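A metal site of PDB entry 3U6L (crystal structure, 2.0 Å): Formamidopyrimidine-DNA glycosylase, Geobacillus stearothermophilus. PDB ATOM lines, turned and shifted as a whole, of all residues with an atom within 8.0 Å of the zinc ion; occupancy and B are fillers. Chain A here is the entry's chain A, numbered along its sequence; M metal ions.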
ATOM      1  N   PHE A 181      24.528  -7.024 -13.849  1.00  0.00           N
ATOM      2  CA  PHE A 181      23.794  -6.872 -12.601  1.00  0.00           C
ATOM      3  C   PHE A 181      24.759  -6.932 -11.421  1.00  0.00           C
ATOM      4  O   PHE A 181      24.728  -6.088 -10.530  1.00  0.00           O
ATOM      5  CB  PHE A 181      22.716  -7.929 -12.418  1.00  0.00           C
ATOM      6  CG  PHE A 181      22.131  -7.938 -11.034  1.00  0.00           C
ATOM      7  CD1 PHE A 181      21.148  -7.024 -10.674  1.00  0.00           C
ATOM      8  CD2 PHE A 181      22.613  -8.812 -10.070  1.00  0.00           C
ATOM      9  CE1 PHE A 181      20.633  -7.005  -9.391  1.00  0.00           C
ATOM     10  CE2 PHE A 181      22.103  -8.805  -8.783  1.00  0.00           C
ATOM     11  CZ  PHE A 181      21.115  -7.900  -8.440  1.00  0.00           C
ATOM     12  N   TYR A 239      20.173 -13.859 -11.093  1.00  0.00           N
ATOM     13  CA  TYR A 239      19.717 -12.637 -10.455  1.00  0.00           C
ATOM     14  C   TYR A 239      18.681 -11.907 -11.294  1.00  0.00           C
ATOM     15  O   TYR A 239      17.703 -11.379 -10.764  1.00  0.00           O
ATOM     16  CB  TYR A 239      20.893 -11.695 -10.170  1.00  0.00           C
ATOM     17  CG  TYR A 239      21.780 -12.144  -9.039  1.00  0.00           C
ATOM     18  CD1 TYR A 239      23.033 -12.706  -9.286  1.00  0.00           C
ATOM     19  CD2 TYR A 239      21.365 -12.024  -7.718  1.00  0.00           C
ATOM     20  CE1 TYR A 239      23.844 -13.125  -8.250  1.00  0.00           C
ATOM     21  CE2 TYR A 239      22.180 -12.439  -6.674  1.00  0.00           C
ATOM     22  CZ  TYR A 239      23.412 -12.993  -6.940  1.00  0.00           C
ATOM     23  OH  TYR A 239      24.223 -13.412  -5.904  1.00  0.00           O
ATOM     24  N   VAL A 240      18.887 -11.883 -12.611  1.00  0.00           N
ATOM     25  CA  VAL A 240      18.025 -11.092 -13.479  1.00  0.00           C
ATOM     26  C   VAL A 240      17.493 -11.836 -14.696  1.00  0.00           C
ATOM     27  O   VAL A 240      16.351 -11.637 -15.102  1.00  0.00           O
ATOM     28  CB  VAL A 240      18.715  -9.782 -13.922  1.00  0.00           C
ATOM     29  CG1 VAL A 240      19.010  -8.902 -12.709  1.00  0.00           C
ATOM     30  CG2 VAL A 240      20.001 -10.089 -14.690  1.00  0.00           C
ATOM     31  N   PRO A 247      10.697  -9.952  -8.058  1.00  0.00           N
ATOM     32  CA  PRO A 247      11.506  -9.088  -7.204  1.00  0.00           C
ATOM     33  C   PRO A 247      12.990  -9.377  -7.328  1.00  0.00           C
ATOM     34  O   PRO A 247      13.398 -10.542  -7.378  1.00  0.00           O
ATOM     35  CB  PRO A 247      11.020  -9.419  -5.794  1.00  0.00           C
ATOM     36  CG  PRO A 247      10.391 -10.769  -5.906  1.00  0.00           C
ATOM     37  CD  PRO A 247       9.791 -10.811  -7.269  1.00  0.00           C
ATOM     38  N   CYS A 248      13.788  -8.319  -7.401  1.00  0.00           N
ATOM     39  CA  CYS A 248      15.238  -8.450  -7.356  1.00  0.00           C
ATOM     40  C   CYS A 248      15.605  -9.160  -6.063  1.00  0.00           C
ATOM     41  O   CYS A 248      15.035  -8.887  -5.004  1.00  0.00           O
ATOM     42  CB  CYS A 248      15.906  -7.074  -7.406  1.00  0.00           C
ATOM     43  SG  CYS A 248      17.698  -7.132  -7.161  1.00  0.00           S
ATOM     44  N   LYS A 249      16.574 -10.074  -6.154  1.00  0.00           N
ATOM     45  CA  LYS A 249      16.989 -10.856  -5.009  1.00  0.00           C
ATOM     46  C   LYS A 249      17.833 -10.040  -4.036  1.00  0.00           C
ATOM     47  O   LYS A 249      18.051 -10.452  -2.905  1.00  0.00           O
ATOM     48  CB  LYS A 249      17.790 -12.082  -5.480  1.00  0.00           C
ATOM     49  CG  LYS A 249      16.978 -13.039  -6.342  1.00  0.00           C
ATOM     50  CD  LYS A 249      17.788 -14.264  -6.732  1.00  0.00           C
ATOM     51  CE  LYS A 249      16.933 -15.260  -7.509  1.00  0.00           C
ATOM     52  NZ  LYS A 249      17.673 -16.523  -7.756  1.00  0.00           N
ATOM     53  N   ARG A 250      18.295  -8.869  -4.483  1.00  0.00           N
ATOM     54  CA  ARG A 250      19.114  -8.034  -3.607  1.00  0.00           C
ATOM     55  C   ARG A 250      18.386  -6.825  -3.024  1.00  0.00           C
ATOM     56  O   ARG A 250      18.707  -6.382  -1.922  1.00  0.00           O
ATOM     57  CB  ARG A 250      20.400  -7.598  -4.329  1.00  0.00           C
ATOM     58  CG  ARG A 250      21.365  -8.739  -4.525  1.00  0.00           C
ATOM     59  CD  ARG A 250      22.742  -8.267  -4.918  1.00  0.00           C
ATOM     60  NE  ARG A 250      23.695  -9.364  -4.929  1.00  0.00           N
ATOM     61  CZ  ARG A 250      24.872  -9.323  -5.542  1.00  0.00           C
ATOM     62  NH1 ARG A 250      25.236  -8.230  -6.197  1.00  0.00           N
ATOM     63  NH2 ARG A 250      25.674 -10.374  -5.506  1.00  0.00           N
ATOM     64  N   CYS A 251      17.397  -6.295  -3.750  1.00  0.00           N
ATOM     65  CA  CYS A 251      16.689  -5.113  -3.268  1.00  0.00           C
ATOM     66  C   CYS A 251      15.159  -5.181  -3.331  1.00  0.00           C
ATOM     67  O   CYS A 251      14.474  -4.318  -2.808  1.00  0.00           O
ATOM     68  CB  CYS A 251      17.160  -3.875  -4.019  1.00  0.00           C
ATOM     69  SG  CYS A 251      16.493  -3.733  -5.695  1.00  0.00           S
ATOM     70  N   GLY A 252      14.626  -6.215  -3.985  1.00  0.00           N
ATOM     71  CA  GLY A 252      13.182  -6.408  -4.027  1.00  0.00           C
ATOM     72  C   GLY A 252      12.435  -5.630  -5.101  1.00  0.00           C
ATOM     73  O   GLY A 252      11.221  -5.789  -5.251  1.00  0.00           O
ATOM     74  N   THR A 253      13.141  -4.797  -5.847  1.00  0.00           N
ATOM     75  CA  THR A 253      12.546  -4.063  -6.968  1.00  0.00           C
ATOM     76  C   THR A 253      12.247  -5.033  -8.107  1.00  0.00           C
ATOM     77  O   THR A 253      13.057  -5.901  -8.413  1.00  0.00           O
ATOM     78  CB  THR A 253      13.508  -2.981  -7.479  1.00  0.00           C
ATOM     79  OG1 THR A 253      13.874  -2.107  -6.398  1.00  0.00           O
ATOM     80  CG2 THR A 253      12.874  -2.168  -8.603  1.00  0.00           C
ATOM     81  N   PRO A 254      11.069  -4.899  -8.740  1.00  0.00           N
ATOM     82  CA  PRO A 254      10.749  -5.777  -9.872  1.00  0.00           C
ATOM     83  C   PRO A 254      11.816  -5.711 -10.958  1.00  0.00           C
ATOM     84  O   PRO A 254      12.181  -4.618 -11.410  1.00  0.00           O
ATOM     85  CB  PRO A 254       9.422  -5.205 -10.393  1.00  0.00           C
ATOM     86  CG  PRO A 254       8.807  -4.541  -9.190  1.00  0.00           C
ATOM     87  CD  PRO A 254       9.966  -3.963  -8.440  1.00  0.00           C
ATOM     88  N   ILE A 255      12.317  -6.872 -11.371  1.00  0.00           N
ATOM     89  CA  ILE A 255      13.243  -6.921 -12.485  1.00  0.00           C
ATOM     90  C   ILE A 255      12.502  -6.510 -13.748  1.00  0.00           C
ATOM     91  O   ILE A 255      11.346  -6.875 -13.954  1.00  0.00           O
ATOM     92  CB  ILE A 255      13.833  -8.341 -12.661  1.00  0.00           C
ATOM     93  CG1 ILE A 255      14.636  -8.718 -11.404  1.00  0.00           C
ATOM     94  CG2 ILE A 255      14.715  -8.422 -13.921  1.00  0.00           C
ATOM     95  CD1 ILE A 255      15.669  -7.661 -11.005  1.00  0.00           C
ATOM     96  N   TYR A 267      17.381  -6.494 -16.124  1.00  0.00           N
ATOM     97  CA  TYR A 267      18.163  -5.703 -15.185  1.00  0.00           C
ATOM     98  C   TYR A 267      17.306  -5.216 -14.033  1.00  0.00           C
ATOM     99  O   TYR A 267      16.076  -5.178 -14.114  1.00  0.00           O
ATOM    100  CB  TYR A 267      18.766  -4.500 -15.909  1.00  0.00           C
ATOM    101  CG  TYR A 267      17.705  -3.590 -16.487  1.00  0.00           C
ATOM    102  CD1 TYR A 267      17.258  -2.479 -15.781  1.00  0.00           C
ATOM    103  CD2 TYR A 267      17.131  -3.855 -17.729  1.00  0.00           C
ATOM    104  CE1 TYR A 267      16.272  -1.657 -16.293  1.00  0.00           C
ATOM    105  CE2 TYR A 267      16.146  -3.030 -18.255  1.00  0.00           C
ATOM    106  CZ  TYR A 267      15.728  -1.931 -17.530  1.00  0.00           C
ATOM    107  OH  TYR A 267      14.751  -1.114 -18.043  1.00  0.00           O
ATOM    108  N   CYS A 268      17.972  -4.869 -12.931  1.00  0.00           N
ATOM    109  CA  CYS A 268      17.303  -4.200 -11.829  1.00  0.00           C
ATOM    110  C   CYS A 268      17.579  -2.712 -11.955  1.00  0.00           C
ATOM    111  O   CYS A 268      18.742  -2.289 -11.939  1.00  0.00           O
ATOM    112  CB  CYS A 268      17.823  -4.709 -10.488  1.00  0.00           C
ATOM    113  SG  CYS A 268      17.080  -3.804  -9.112  1.00  0.00           S
ATOM    114  N   PRO A 269      16.517  -1.910 -12.079  1.00  0.00           N
ATOM    115  CA  PRO A 269      16.665  -0.461 -12.265  1.00  0.00           C
ATOM    116  C   PRO A 269      17.156   0.235 -10.994  1.00  0.00           C
ATOM    117  O   PRO A 269      17.479   1.422 -11.060  1.00  0.00           O
ATOM    118  CB  PRO A 269      15.253  -0.007 -12.619  1.00  0.00           C
ATOM    119  CG  PRO A 269      14.372  -0.989 -11.953  1.00  0.00           C
ATOM    120  CD  PRO A 269      15.102  -2.311 -12.033  1.00  0.00           C
ATOM    121  N   ARG A 270      17.191  -0.469  -9.875  1.00  0.00           N
ATOM    122  CA  ARG A 270      17.729   0.129  -8.641  1.00  0.00           C
ATOM    123  C   ARG A 270      19.198  -0.253  -8.409  1.00  0.00           C
ATOM    124  O   ARG A 270      20.026   0.607  -8.137  1.00  0.00           O
ATOM    125  CB  ARG A 270      16.881  -0.249  -7.425  1.00  0.00           C
ATOM    126  CG  ARG A 270      17.429   0.283  -6.113  1.00  0.00           C
ATOM    127  CD  ARG A 270      16.502  -0.020  -4.929  1.00  0.00           C
ATOM    128  NE  ARG A 270      17.000   0.611  -3.710  1.00  0.00           N
ATOM    129  CZ  ARG A 270      16.368   0.603  -2.536  1.00  0.00           C
ATOM    130  NH1 ARG A 270      16.914   1.218  -1.495  1.00  0.00           N
ATOM    131  NH2 ARG A 270      15.201  -0.019  -2.396  1.00  0.00           N
ATOM    132  N   CYS A 271      19.497  -1.552  -8.513  1.00  0.00           N
ATOM    133  CA  CYS A 271      20.858  -2.050  -8.308  1.00  0.00           C
ATOM    134  C   CYS A 271      21.825  -1.603  -9.392  1.00  0.00           C
ATOM    135  O   CYS A 271      23.010  -1.412  -9.140  1.00  0.00           O
ATOM    136  CB  CYS A 271      20.872  -3.580  -8.214  1.00  0.00           C
ATOM    137  SG  CYS A 271      20.193  -4.259  -6.661  1.00  0.00           S
ATOM    138  N   GLN A 272      21.322  -1.444 -10.612  1.00  0.00           N
ATOM    139  CA  GLN A 272      22.188  -1.077 -11.722  1.00  0.00           C
ATOM    140  C   GLN A 272      22.021   0.375 -12.112  1.00  0.00           C
ATOM    141  O   GLN A 272      20.906   0.877 -12.162  1.00  0.00           O
ATOM    142  CB  GLN A 272      21.930  -1.998 -12.916  1.00  0.00           C
ATOM    143  CG  GLN A 272      22.287  -3.434 -12.609  1.00  0.00           C
ATOM    144  CD  GLN A 272      21.752  -4.387 -13.629  1.00  0.00           C
ATOM    145  OE1 GLN A 272      20.811  -5.126 -13.371  1.00  0.00           O
ATOM    146  NE2 GLN A 272      22.377  -4.413 -14.818  1.00  0.00           N
HETATM  147 ZN    ZN M   1      17.977  -4.747  -7.204  1.00  0.00          ZN
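The backbone NH (N) of Arg 270 lies close to the side-chain sulfur (SG) of Cys 268, 3.4 Å away.
OE1 of Gln 272 sits at hydrogen-bond distance from N of Cys 268 (2.9 Å).
The side-chain hydroxyl of Thr 253 sits close to the side-chain sulfur of Cys 251, 3.2 Å away.
SG of Cys 248 lies close to N of Arg 250, at 3.2 Å.
N of Cys 248 is in hydrogen-bond range of O of Thr 253, at 2.7 Å.
Along chain A the residues within 4 Å of the zinc ion span positions 248 to 271.
The zinc ion is bound by SG of Cys 268, SG of Cys 271, SG of Cys 251 and SG of Cys 248.
The zinc ion has four donor atoms within binding distance.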
